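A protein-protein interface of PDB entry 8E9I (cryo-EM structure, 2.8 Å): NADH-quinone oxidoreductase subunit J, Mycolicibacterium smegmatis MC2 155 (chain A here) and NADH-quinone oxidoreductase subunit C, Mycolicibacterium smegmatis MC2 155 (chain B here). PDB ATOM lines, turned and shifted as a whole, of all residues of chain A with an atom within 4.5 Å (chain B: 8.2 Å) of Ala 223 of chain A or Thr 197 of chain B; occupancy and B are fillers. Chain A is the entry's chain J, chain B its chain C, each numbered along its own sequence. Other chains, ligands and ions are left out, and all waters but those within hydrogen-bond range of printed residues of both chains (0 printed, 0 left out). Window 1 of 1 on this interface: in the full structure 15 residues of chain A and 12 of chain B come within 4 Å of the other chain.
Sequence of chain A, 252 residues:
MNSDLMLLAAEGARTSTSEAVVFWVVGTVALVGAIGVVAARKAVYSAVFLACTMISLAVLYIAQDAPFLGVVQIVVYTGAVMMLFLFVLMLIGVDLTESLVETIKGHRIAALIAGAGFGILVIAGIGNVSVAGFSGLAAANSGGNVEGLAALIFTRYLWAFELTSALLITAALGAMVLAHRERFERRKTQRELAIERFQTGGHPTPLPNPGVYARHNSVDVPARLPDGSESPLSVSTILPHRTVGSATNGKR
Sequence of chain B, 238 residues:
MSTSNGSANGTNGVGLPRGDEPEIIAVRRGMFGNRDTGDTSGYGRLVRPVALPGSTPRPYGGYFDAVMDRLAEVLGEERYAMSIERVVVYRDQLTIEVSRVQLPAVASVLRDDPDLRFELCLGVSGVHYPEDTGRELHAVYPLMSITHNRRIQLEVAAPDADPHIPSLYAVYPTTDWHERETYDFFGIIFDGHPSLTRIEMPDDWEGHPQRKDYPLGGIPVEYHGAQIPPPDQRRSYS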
ATOM      1  N   PRO A 208      28.280 -21.480   4.686  1.00  0.00           N
ATOM      2  CA  PRO A 208      26.926 -21.825   5.119  1.00  0.00           C
ATOM      3  C   PRO A 208      26.393 -20.805   6.112  1.00  0.00           C
ATOM      4  O   PRO A 208      27.122 -20.260   6.942  1.00  0.00           O
ATOM      5  CB  PRO A 208      27.094 -23.205   5.765  1.00  0.00           C
ATOM      6  CG  PRO A 208      28.542 -23.322   6.058  1.00  0.00           C
ATOM      7  CD  PRO A 208      29.240 -22.546   4.999  1.00  0.00           C
ATOM      8  N   ASN A 209      25.115 -20.536   5.998  1.00  0.00           N
ATOM      9  CA  ASN A 209      24.460 -19.536   6.820  1.00  0.00           C
ATOM     10  C   ASN A 209      24.354 -20.002   8.262  1.00  0.00           C
ATOM     11  O   ASN A 209      24.352 -21.203   8.538  1.00  0.00           O
ATOM     12  CB  ASN A 209      23.065 -19.251   6.281  1.00  0.00           C
ATOM     13  CG  ASN A 209      22.184 -20.481   6.279  1.00  0.00           C
ATOM     14  OD1 ASN A 209      22.624 -21.575   5.931  1.00  0.00           O
ATOM     15  ND2 ASN A 209      20.943 -20.315   6.706  1.00  0.00           N
ATOM     16  N   GLY A 211      22.442 -21.071  11.558  1.00  0.00           N
ATOM     17  CA  GLY A 211      21.228 -21.847  11.641  1.00  0.00           C
ATOM     18  C   GLY A 211      20.036 -21.007  12.051  1.00  0.00           C
ATOM     19  O   GLY A 211      20.161 -19.977  12.709  1.00  0.00           O
ATOM     20  N   TYR A 213      16.499 -21.474  14.074  1.00  0.00           N
ATOM     21  CA  TYR A 213      15.742 -22.309  14.986  1.00  0.00           C
ATOM     22  C   TYR A 213      14.521 -21.537  15.445  1.00  0.00           C
ATOM     23  O   TYR A 213      14.492 -20.307  15.387  1.00  0.00           O
ATOM     24  CB  TYR A 213      16.565 -22.706  16.208  1.00  0.00           C
ATOM     25  CG  TYR A 213      17.785 -23.526  15.902  1.00  0.00           C
ATOM     26  CD1 TYR A 213      18.871 -22.971  15.254  1.00  0.00           C
ATOM     27  CD2 TYR A 213      17.857 -24.853  16.280  1.00  0.00           C
ATOM     28  CE1 TYR A 213      19.985 -23.715  14.977  1.00  0.00           C
ATOM     29  CE2 TYR A 213      18.968 -25.607  16.006  1.00  0.00           C
ATOM     30  CZ  TYR A 213      20.033 -25.033  15.357  1.00  0.00           C
ATOM     31  OH  TYR A 213      21.153 -25.780  15.081  1.00  0.00           O
ATOM     32  N   VAL A 221      23.908 -18.113  15.951  1.00  0.00           N
ATOM     33  CA  VAL A 221      23.359 -19.457  16.096  1.00  0.00           C
ATOM     34  C   VAL A 221      24.032 -20.401  15.104  1.00  0.00           C
ATOM     35  O   VAL A 221      23.917 -20.194  13.890  1.00  0.00           O
ATOM     36  CB  VAL A 221      21.839 -19.439  15.885  1.00  0.00           C
ATOM     37  CG1 VAL A 221      21.261 -20.825  16.066  1.00  0.00           C
ATOM     38  CG2 VAL A 221      21.185 -18.443  16.827  1.00  0.00           C
ATOM     39  N   PRO A 222      24.727 -21.446  15.554  1.00  0.00           N
ATOM     40  CA  PRO A 222      25.352 -22.367  14.599  1.00  0.00           C
ATOM     41  C   PRO A 222      24.339 -23.326  13.997  1.00  0.00           C
ATOM     42  O   PRO A 222      23.365 -23.719  14.644  1.00  0.00           O
ATOM     43  CB  PRO A 222      26.385 -23.106  15.453  1.00  0.00           C
ATOM     44  CG  PRO A 222      25.798 -23.108  16.803  1.00  0.00           C
ATOM     45  CD  PRO A 222      25.048 -21.810  16.944  1.00  0.00           C
ATOM     46  N   ALA A 223      24.584 -23.713  12.751  1.00  0.00           N
ATOM     47  CA  ALA A 223      23.679 -24.598  12.035  1.00  0.00           C
ATOM     48  C   ALA A 223      23.900 -26.047  12.449  1.00  0.00           C
ATOM     49  O   ALA A 223      24.944 -26.404  12.997  1.00  0.00           O
ATOM     50  CB  ALA A 223      23.872 -24.451  10.528  1.00  0.00           C
ATOM     51  N   ARG A 224      22.902 -26.883  12.180  1.00  0.00           N
ATOM     52  CA  ARG A 224      22.916 -28.274  12.614  1.00  0.00           C
ATOM     53  C   ARG A 224      23.235 -29.197  11.446  1.00  0.00           C
ATOM     54  O   ARG A 224      22.541 -29.180  10.425  1.00  0.00           O
ATOM     55  CB  ARG A 224      21.569 -28.654  13.224  1.00  0.00           C
ATOM     56  CG  ARG A 224      21.500 -30.084  13.722  1.00  0.00           C
ATOM     57  CD  ARG A 224      20.138 -30.394  14.306  1.00  0.00           C
ATOM     58  NE  ARG A 224      19.909 -29.677  15.553  1.00  0.00           N
ATOM     59  CZ  ARG A 224      18.711 -29.399  16.050  1.00  0.00           C
ATOM     60  NH1 ARG A 224      17.603 -29.781  15.440  1.00  0.00           N
ATOM     61  NH2 ARG A 224      18.626 -28.721  17.191  1.00  0.00           N
ATOM     62  N   LEU A 225      24.273 -30.008  11.609  1.00  0.00           N
ATOM     63  CA  LEU A 225      24.647 -31.010  10.622  1.00  0.00           C
ATOM     64  C   LEU A 225      23.717 -32.211  10.725  1.00  0.00           C
ATOM     65  O   LEU A 225      22.999 -32.374  11.711  1.00  0.00           O
ATOM     66  CB  LEU A 225      26.101 -31.417  10.836  1.00  0.00           C
ATOM     67  CG  LEU A 225      27.103 -30.371  10.350  1.00  0.00           C
ATOM     68  CD1 LEU A 225      28.481 -30.601  10.930  1.00  0.00           C
ATOM     69  CD2 LEU A 225      27.169 -30.385   8.833  1.00  0.00           C
ATOM     70  N   SER A 229      25.171 -32.499  15.180  1.00  0.00           N
ATOM     71  CA  SER A 229      26.222 -31.634  15.685  1.00  0.00           C
ATOM     72  C   SER A 229      26.087 -30.238  15.084  1.00  0.00           C
ATOM     73  O   SER A 229      25.343 -30.010  14.128  1.00  0.00           O
ATOM     74  CB  SER A 229      27.596 -32.210  15.356  1.00  0.00           C
ATOM     75  OG  SER A 229      27.869 -32.083  13.975  1.00  0.00           O
ATOM     76  N   GLU A 230      26.832 -29.296  15.652  1.00  0.00           N
ATOM     77  CA  GLU A 230      26.797 -27.905  15.225  1.00  0.00           C
ATOM     78  C   GLU A 230      27.918 -27.670  14.226  1.00  0.00           C
ATOM     79  O   GLU A 230      29.084 -27.948  14.519  1.00  0.00           O
ATOM     80  CB  GLU A 230      26.934 -26.965  16.422  1.00  0.00           C
ATOM     81  N   SER A 231      27.570 -27.162  13.056  1.00  0.00           N
ATOM     82  CA  SER A 231      28.569 -26.913  12.029  1.00  0.00           C
ATOM     83  C   SER A 231      29.428 -25.720  12.428  1.00  0.00           C
ATOM     84  O   SER A 231      28.896 -24.617  12.593  1.00  0.00           O
ATOM     85  CB  SER A 231      27.899 -26.653  10.689  1.00  0.00           C
ATOM     86  OG  SER A 231      26.907 -25.655  10.814  1.00  0.00           O
ATOM     87  N   SER A 234      29.133 -22.669   9.825  1.00  0.00           N
ATOM     88  CA  SER A 234      27.922 -21.864   9.728  1.00  0.00           C
ATOM     89  C   SER A 234      28.047 -20.582  10.536  1.00  0.00           C
ATOM     90  O   SER A 234      27.631 -19.511  10.084  1.00  0.00           O
ATOM     91  CB  SER A 234      26.718 -22.674  10.201  1.00  0.00           C
ATOM     92  OG  SER A 234      26.895 -23.099  11.539  1.00  0.00           O
ATOM     93  N   ASP B 176      27.020 -27.442  -4.133  1.00  0.00           N
ATOM     94  CA  ASP B 176      27.006 -27.337  -2.677  1.00  0.00           C
ATOM     95  C   ASP B 176      25.620 -26.982  -2.163  1.00  0.00           C
ATOM     96  O   ASP B 176      25.068 -27.677  -1.305  1.00  0.00           O
ATOM     97  CB  ASP B 176      28.024 -26.296  -2.217  1.00  0.00           C
ATOM     98  N   TRP B 177      25.028 -25.909  -2.683  1.00  0.00           N
ATOM     99  CA  TRP B 177      23.677 -25.565  -2.259  1.00  0.00           C
ATOM    100  C   TRP B 177      22.668 -26.601  -2.714  1.00  0.00           C
ATOM    101  O   TRP B 177      21.793 -26.992  -1.937  1.00  0.00           O
ATOM    102  CB  TRP B 177      23.267 -24.204  -2.797  1.00  0.00           C
ATOM    103  CG  TRP B 177      23.769 -23.065  -2.010  1.00  0.00           C
ATOM    104  CD1 TRP B 177      24.770 -23.080  -1.092  1.00  0.00           C
ATOM    105  CD2 TRP B 177      23.280 -21.726  -2.055  1.00  0.00           C
ATOM    106  NE1 TRP B 177      24.943 -21.827  -0.567  1.00  0.00           N
ATOM    107  CE2 TRP B 177      24.039 -20.978  -1.145  1.00  0.00           C
ATOM    108  CE3 TRP B 177      22.277 -21.087  -2.786  1.00  0.00           C
ATOM    109  CZ2 TRP B 177      23.825 -19.624  -0.941  1.00  0.00           C
ATOM    110  CZ3 TRP B 177      22.067 -19.745  -2.584  1.00  0.00           C
ATOM    111  CH2 TRP B 177      22.837 -19.026  -1.669  1.00  0.00           C
ATOM    112  N   HIS B 178      22.755 -27.048  -3.965  1.00  0.00           N
ATOM    113  CA  HIS B 178      21.800 -28.045  -4.424  1.00  0.00           C
ATOM    114  C   HIS B 178      21.852 -29.272  -3.533  1.00  0.00           C
ATOM    115  O   HIS B 178      20.833 -29.677  -2.961  1.00  0.00           O
ATOM    116  CB  HIS B 178      22.085 -28.414  -5.873  1.00  0.00           C
ATOM    117  CG  HIS B 178      21.918 -27.271  -6.820  1.00  0.00           C
ATOM    118  ND1 HIS B 178      20.702 -26.936  -7.375  1.00  0.00           N
ATOM    119  CD2 HIS B 178      22.811 -26.375  -7.301  1.00  0.00           C
ATOM    120  CE1 HIS B 178      20.856 -25.886  -8.161  1.00  0.00           C
ATOM    121  NE2 HIS B 178      22.126 -25.528  -8.136  1.00  0.00           N
ATOM    122  N   GLU B 179      23.046 -29.828  -3.341  1.00  0.00           N
ATOM    123  CA  GLU B 179      23.187 -30.957  -2.439  1.00  0.00           C
ATOM    124  C   GLU B 179      22.588 -30.647  -1.079  1.00  0.00           C
ATOM    125  O   GLU B 179      22.010 -31.531  -0.441  1.00  0.00           O
ATOM    126  CB  GLU B 179      24.658 -31.338  -2.297  1.00  0.00           C
ATOM    127  N   ARG B 180      22.711 -29.405  -0.617  1.00  0.00           N
ATOM    128  CA  ARG B 180      22.092 -29.051   0.650  1.00  0.00           C
ATOM    129  C   ARG B 180      20.578 -29.112   0.548  1.00  0.00           C
ATOM    130  O   ARG B 180      19.930 -29.825   1.322  1.00  0.00           O
ATOM    131  CB  ARG B 180      22.543 -27.665   1.088  1.00  0.00           C
ATOM    132  CG  ARG B 180      23.923 -27.662   1.685  1.00  0.00           C
ATOM    133  CD  ARG B 180      24.336 -26.277   2.092  1.00  0.00           C
ATOM    134  NE  ARG B 180      23.518 -25.786   3.189  1.00  0.00           N
ATOM    135  CZ  ARG B 180      23.285 -24.507   3.436  1.00  0.00           C
ATOM    136  NH1 ARG B 180      23.792 -23.553   2.675  1.00  0.00           N
ATOM    137  NH2 ARG B 180      22.526 -24.178   4.476  1.00  0.00           N
ATOM    138  N   GLU B 181      19.998 -28.416  -0.428  1.00  0.00           N
ATOM    139  CA  GLU B 181      18.548 -28.442  -0.557  1.00  0.00           C
ATOM    140  C   GLU B 181      18.057 -29.874  -0.671  1.00  0.00           C
ATOM    141  O   GLU B 181      17.159 -30.296   0.066  1.00  0.00           O
ATOM    142  CB  GLU B 181      18.110 -27.618  -1.766  1.00  0.00           C
ATOM    143  N   THR B 182      18.679 -30.656  -1.553  1.00  0.00           N
ATOM    144  CA  THR B 182      18.279 -32.045  -1.704  1.00  0.00           C
ATOM    145  C   THR B 182      18.319 -32.782  -0.377  1.00  0.00           C
ATOM    146  O   THR B 182      17.400 -33.548  -0.073  1.00  0.00           O
ATOM    147  CB  THR B 182      19.172 -32.752  -2.716  1.00  0.00           C
ATOM    148  OG1 THR B 182      20.541 -32.521  -2.390  1.00  0.00           O
ATOM    149  CG2 THR B 182      18.908 -32.220  -4.101  1.00  0.00           C
ATOM    150  N   TYR B 183      19.356 -32.571   0.434  1.00  0.00           N
ATOM    151  CA  TYR B 183      19.348 -33.188   1.753  1.00  0.00           C
ATOM    152  C   TYR B 183      18.149 -32.708   2.549  1.00  0.00           C
ATOM    153  O   TYR B 183      17.323 -33.508   3.000  1.00  0.00           O
ATOM    154  CB  TYR B 183      20.635 -32.876   2.512  1.00  0.00           C
ATOM    155  CG  TYR B 183      20.449 -33.006   4.003  1.00  0.00           C
ATOM    156  CD1 TYR B 183      20.119 -34.223   4.573  1.00  0.00           C
ATOM    157  CD2 TYR B 183      20.571 -31.911   4.839  1.00  0.00           C
ATOM    158  CE1 TYR B 183      19.932 -34.347   5.930  1.00  0.00           C
ATOM    159  CE2 TYR B 183      20.385 -32.028   6.198  1.00  0.00           C
ATOM    160  CZ  TYR B 183      20.065 -33.247   6.734  1.00  0.00           C
ATOM    161  OH  TYR B 183      19.879 -33.370   8.090  1.00  0.00           O
ATOM    162  N   ASP B 184      17.997 -31.389   2.660  1.00  0.00           N
ATOM    163  CA  ASP B 184      16.920 -30.828   3.463  1.00  0.00           C
ATOM    164  C   ASP B 184      15.585 -31.423   3.055  1.00  0.00           C
ATOM    165  O   ASP B 184      14.720 -31.692   3.893  1.00  0.00           O
ATOM    166  CB  ASP B 184      16.889 -29.312   3.292  1.00  0.00           C
ATOM    167  CG  ASP B 184      15.983 -28.642   4.280  1.00  0.00           C
ATOM    168  OD1 ASP B 184      15.512 -29.324   5.209  1.00  0.00           O
ATOM    169  OD2 ASP B 184      15.731 -27.434   4.123  1.00  0.00           O
ATOM    170  N   HIS B 193      30.449 -33.474   1.956  1.00  0.00           N
ATOM    171  CA  HIS B 193      30.069 -32.091   1.749  1.00  0.00           C
ATOM    172  C   HIS B 193      30.559 -31.257   2.931  1.00  0.00           C
ATOM    173  O   HIS B 193      30.483 -31.707   4.077  1.00  0.00           O
ATOM    174  CB  HIS B 193      28.553 -31.983   1.608  1.00  0.00           C
ATOM    175  CG  HIS B 193      28.064 -30.609   1.269  1.00  0.00           C
ATOM    176  ND1 HIS B 193      28.020 -29.585   2.189  1.00  0.00           N
ATOM    177  CD2 HIS B 193      27.582 -30.095   0.114  1.00  0.00           C
ATOM    178  CE1 HIS B 193      27.543 -28.498   1.613  1.00  0.00           C
ATOM    179  NE2 HIS B 193      27.269 -28.781   0.353  1.00  0.00           N
ATOM    180  N   PRO B 194      31.084 -30.054   2.692  1.00  0.00           N
ATOM    181  CA  PRO B 194      31.568 -29.246   3.822  1.00  0.00           C
ATOM    182  C   PRO B 194      30.581 -29.157   4.970  1.00  0.00           C
ATOM    183  O   PRO B 194      30.905 -29.580   6.086  1.00  0.00           O
ATOM    184  CB  PRO B 194      31.819 -27.876   3.184  1.00  0.00           C
ATOM    185  CG  PRO B 194      32.116 -28.181   1.774  1.00  0.00           C
ATOM    186  CD  PRO B 194      31.274 -29.361   1.407  1.00  0.00           C
ATOM    187  N   SER B 195      29.381 -28.638   4.735  1.00  0.00           N
ATOM    188  CA  SER B 195      28.379 -28.562   5.787  1.00  0.00           C
ATOM    189  C   SER B 195      26.986 -28.773   5.215  1.00  0.00           C
ATOM    190  O   SER B 195      26.421 -27.872   4.591  1.00  0.00           O
ATOM    191  CB  SER B 195      28.454 -27.216   6.501  1.00  0.00           C
ATOM    192  OG  SER B 195      29.688 -27.072   7.177  1.00  0.00           O
ATOM    193  N   LEU B 196      26.427 -29.963   5.422  1.00  0.00           N
ATOM    194  CA  LEU B 196      25.059 -30.253   5.005  1.00  0.00           C
ATOM    195  C   LEU B 196      24.066 -29.694   6.021  1.00  0.00           C
ATOM    196  O   LEU B 196      23.419 -30.414   6.779  1.00  0.00           O
ATOM    197  CB  LEU B 196      24.860 -31.748   4.821  1.00  0.00           C
ATOM    198  CG  LEU B 196      25.262 -32.300   3.465  1.00  0.00           C
ATOM    199  CD1 LEU B 196      25.180 -33.804   3.496  1.00  0.00           C
ATOM    200  CD2 LEU B 196      24.374 -31.736   2.370  1.00  0.00           C
ATOM    201  N   THR B 197      23.965 -28.375   6.029  1.00  0.00           N
ATOM    202  CA  THR B 197      22.938 -27.720   6.811  1.00  0.00           C
ATOM    203  C   THR B 197      21.708 -27.494   5.946  1.00  0.00           C
ATOM    204  O   THR B 197      21.808 -27.255   4.742  1.00  0.00           O
ATOM    205  CB  THR B 197      23.445 -26.387   7.357  1.00  0.00           C
ATOM    206  OG1 THR B 197      23.657 -25.474   6.274  1.00  0.00           O
ATOM    207  CG2 THR B 197      24.752 -26.581   8.106  1.00  0.00           C
ATOM    208  N   ARG B 198      20.539 -27.588   6.568  1.00  0.00           N
ATOM    209  CA  ARG B 198      19.319 -27.252   5.860  1.00  0.00           C
ATOM    210  C   ARG B 198      19.410 -25.830   5.323  1.00  0.00           C
ATOM    211  O   ARG B 198      19.876 -24.910   5.998  1.00  0.00           O
ATOM    212  CB  ARG B 198      18.110 -27.390   6.776  1.00  0.00           C
ATOM    213  CG  ARG B 198      17.794 -28.814   7.150  1.00  0.00           C
ATOM    214  CD  ARG B 198      16.562 -28.882   8.006  1.00  0.00           C
ATOM    215  NE  ARG B 198      16.266 -30.245   8.426  1.00  0.00           N
ATOM    216  CZ  ARG B 198      15.346 -31.027   7.876  1.00  0.00           C
ATOM    217  NH1 ARG B 198      14.611 -30.624   6.852  1.00  0.00           N
ATOM    218  NH2 ARG B 198      15.155 -32.246   8.369  1.00  0.00           N
ATOM    219  N   ILE B 199      18.962 -25.657   4.084  1.00  0.00           N
ATOM    220  CA  ILE B 199      19.080 -24.366   3.423  1.00  0.00           C
ATOM    221  C   ILE B 199      17.706 -23.716   3.337  1.00  0.00           C
ATOM    222  O   ILE B 199      17.559 -22.522   3.612  1.00  0.00           O
ATOM    223  CB  ILE B 199      19.731 -24.516   2.036  1.00  0.00           C
ATOM    224  CG1 ILE B 199      20.006 -23.144   1.428  1.00  0.00           C
ATOM    225  CG2 ILE B 199      18.857 -25.331   1.106  1.00  0.00           C
ATOM    226  CD1 ILE B 199      20.963 -23.187   0.271  1.00  0.00           C
ATOM    227  N   GLU B 200      16.687 -24.497   2.981  1.00  0.00           N
ATOM    228  CA  GLU B 200      15.335 -23.970   2.827  1.00  0.00           C
ATOM    229  C   GLU B 200      14.564 -23.991   4.143  1.00  0.00           C
ATOM    230  O   GLU B 200      13.977 -22.981   4.539  1.00  0.00           O
ATOM    231  CB  GLU B 200      14.577 -24.765   1.758  1.00  0.00           C
ATOM    232  CG  GLU B 200      15.092 -24.543   0.348  1.00  0.00           C
ATOM    233  CD  GLU B 200      14.832 -23.148  -0.154  1.00  0.00           C
ATOM    234  OE1 GLU B 200      13.925 -22.486   0.376  1.00  0.00           O
ATOM    235  OE2 GLU B 200      15.540 -22.711  -1.081  1.00  0.00           O
ATOM    236  N   MET B 201      14.557 -25.129   4.823  1.00  0.00           N
ATOM    237  CA  MET B 201      13.758 -25.281   6.021  1.00  0.00           C
ATOM    238  C   MET B 201      14.572 -24.926   7.261  1.00  0.00           C
ATOM    239  O   MET B 201      15.803 -24.932   7.233  1.00  0.00           O
ATOM    240  CB  MET B 201      13.247 -26.712   6.127  1.00  0.00           C
ATOM    241  CG  MET B 201      12.200 -27.086   5.085  1.00  0.00           C
ATOM    242  SD  MET B 201      10.966 -25.811   4.768  1.00  0.00           S
ATOM    243  CE  MET B 201       9.839 -26.062   6.129  1.00  0.00           C
ATOM    244  N   PRO B 202      13.906 -24.607   8.369  1.00  0.00           N
ATOM    245  CA  PRO B 202      14.641 -24.273   9.592  1.00  0.00           C
ATOM    246  C   PRO B 202      15.472 -25.447  10.079  1.00  0.00           C
ATOM    247  O   PRO B 202      15.115 -26.611   9.889  1.00  0.00           O
ATOM    248  CB  PRO B 202      13.531 -23.924  10.589  1.00  0.00           C
ATOM    249  CG  PRO B 202      12.362 -23.584   9.753  1.00  0.00           C
ATOM    250  CD  PRO B 202      12.455 -24.456   8.550  1.00  0.00           C
ATOM    251  N   ASP B 203      16.596 -25.128  10.720  1.00  0.00           N
ATOM    252  CA  ASP B 203      17.495 -26.176  11.192  1.00  0.00           C
ATOM    253  C   ASP B 203      16.792 -27.123  12.152  1.00  0.00           C
ATOM    254  O   ASP B 203      17.121 -28.312  12.202  1.00  0.00           O
ATOM    255  CB  ASP B 203      18.715 -25.552  11.864  1.00  0.00           C
ATOM    256  N   ASP B 204      15.820 -26.624  12.908  1.00  0.00           N
ATOM    257  CA  ASP B 204      15.099 -27.441  13.873  1.00  0.00           C
ATOM    258  C   ASP B 204      13.920 -28.177  13.255  1.00  0.00           C
ATOM    259  O   ASP B 204      13.183 -28.850  13.979  1.00  0.00           O
ATOM    260  CB  ASP B 204      14.612 -26.566  15.032  1.00  0.00           C
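The side-chain amide oxygen of Asn 209 of chain A sits at hydrogen-bond distance from the guanidinium group of Arg 180 of chain B (3.0 Å).
The guanidinium group (NH2) of Arg 180 of chain B lies within hydrogen-bond range of the side-chain hydroxyl (OG1) of Thr 197 of chain B, 2.5 Å away. The side-chain hydroxyl (OG) of Ser 231 of chain A sits at hydrogen-bond distance from the side-chain hydroxyl (OG) of Ser 234 of chain A. N of Ser 231 of chain A lies within hydrogen-bond range of O of Ala 223 of chain A (2.7 Å). O of Pro 222 of chain A is in hydrogen-bond range of OH of Tyr 213 of chain A, at 3.1 Å. The backbone NH of Ser 195 of chain B is in hydrogen-bond range of a ring nitrogen (ND1) of His 193 of chain B (3.0 Å). The side-chain hydroxyl (OG) of Ser 234 of chain A is in hydrogen-bond range of the backbone NH (N) of Ala 223 of chain A (2.7 Å).
CG of Pro 208 of chain A touches CB of Ser 195 of chain B, 3.9 Å away. Asp 203 of chain B touches Tyr 213 of chain A. CB of Asp 204 of chain B touches CD2 of Tyr 213 of chain A, 3.9 Å away. Ala 223 of chain A touches Thr 197 of chain B. Arg 224 of chain A touches Thr 197 of chain B. NH1 of Arg 224 of chain A touches O of Asp 203 of chain B, 3.6 Å away. Asp 204 of chain B touches Arg 224 of chain A. Ser 195 of chain B touches Leu 225 of chain A. Leu 225 of chain A touches Leu 196 of chain B (CD2 to N, 3.5 Å). CG2 of Thr 197 of chain B touches OG of Ser 231 of chain A, 3.6 Å away.
Ala 223 of chain A touches just one residue of chain B: Thr 197. Of chain A, only Ala 223 (3.3 Å), Arg 224 (3.9 Å) and Ser 231 (3.6 Å) come within 4 Å of Thr 197 of chain B. Of the printed residues of chain B, Tyr 213 of chain A touches Asp 203 (3.8 Å) and Asp 204 (3.9 Å). Printed residues of chain A within 4 Å of Asp 203 of chain B: Tyr 213 and Arg 224. Of the printed residues of chain B, Ser 231 of chain A touches Ser 195 and Thr 197. Asp 176 of chain B touches none of the printed residues of chain A. Arg 198 of chain B touches none of the printed residues of chain A. The nearest residue of chain B that does not touch Ala 223 of chain A is Asp 203 of chain B (5.1 Å). The nearest residue of chain A that does not touch Thr 197 of chain B is Asn 209 of chain A (4.05 Å).
Of the 13 printed residues of chain A, 7 touch a printed residue of chain B. Hydrophobic or aromatic side chains of chain A within 4 Å of the printed part of chain B: Pro 208, Tyr 213, Ala 223 and Leu 225. Along chain A the printed residues that touch a printed residue of chain B span positions 208 to 231.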
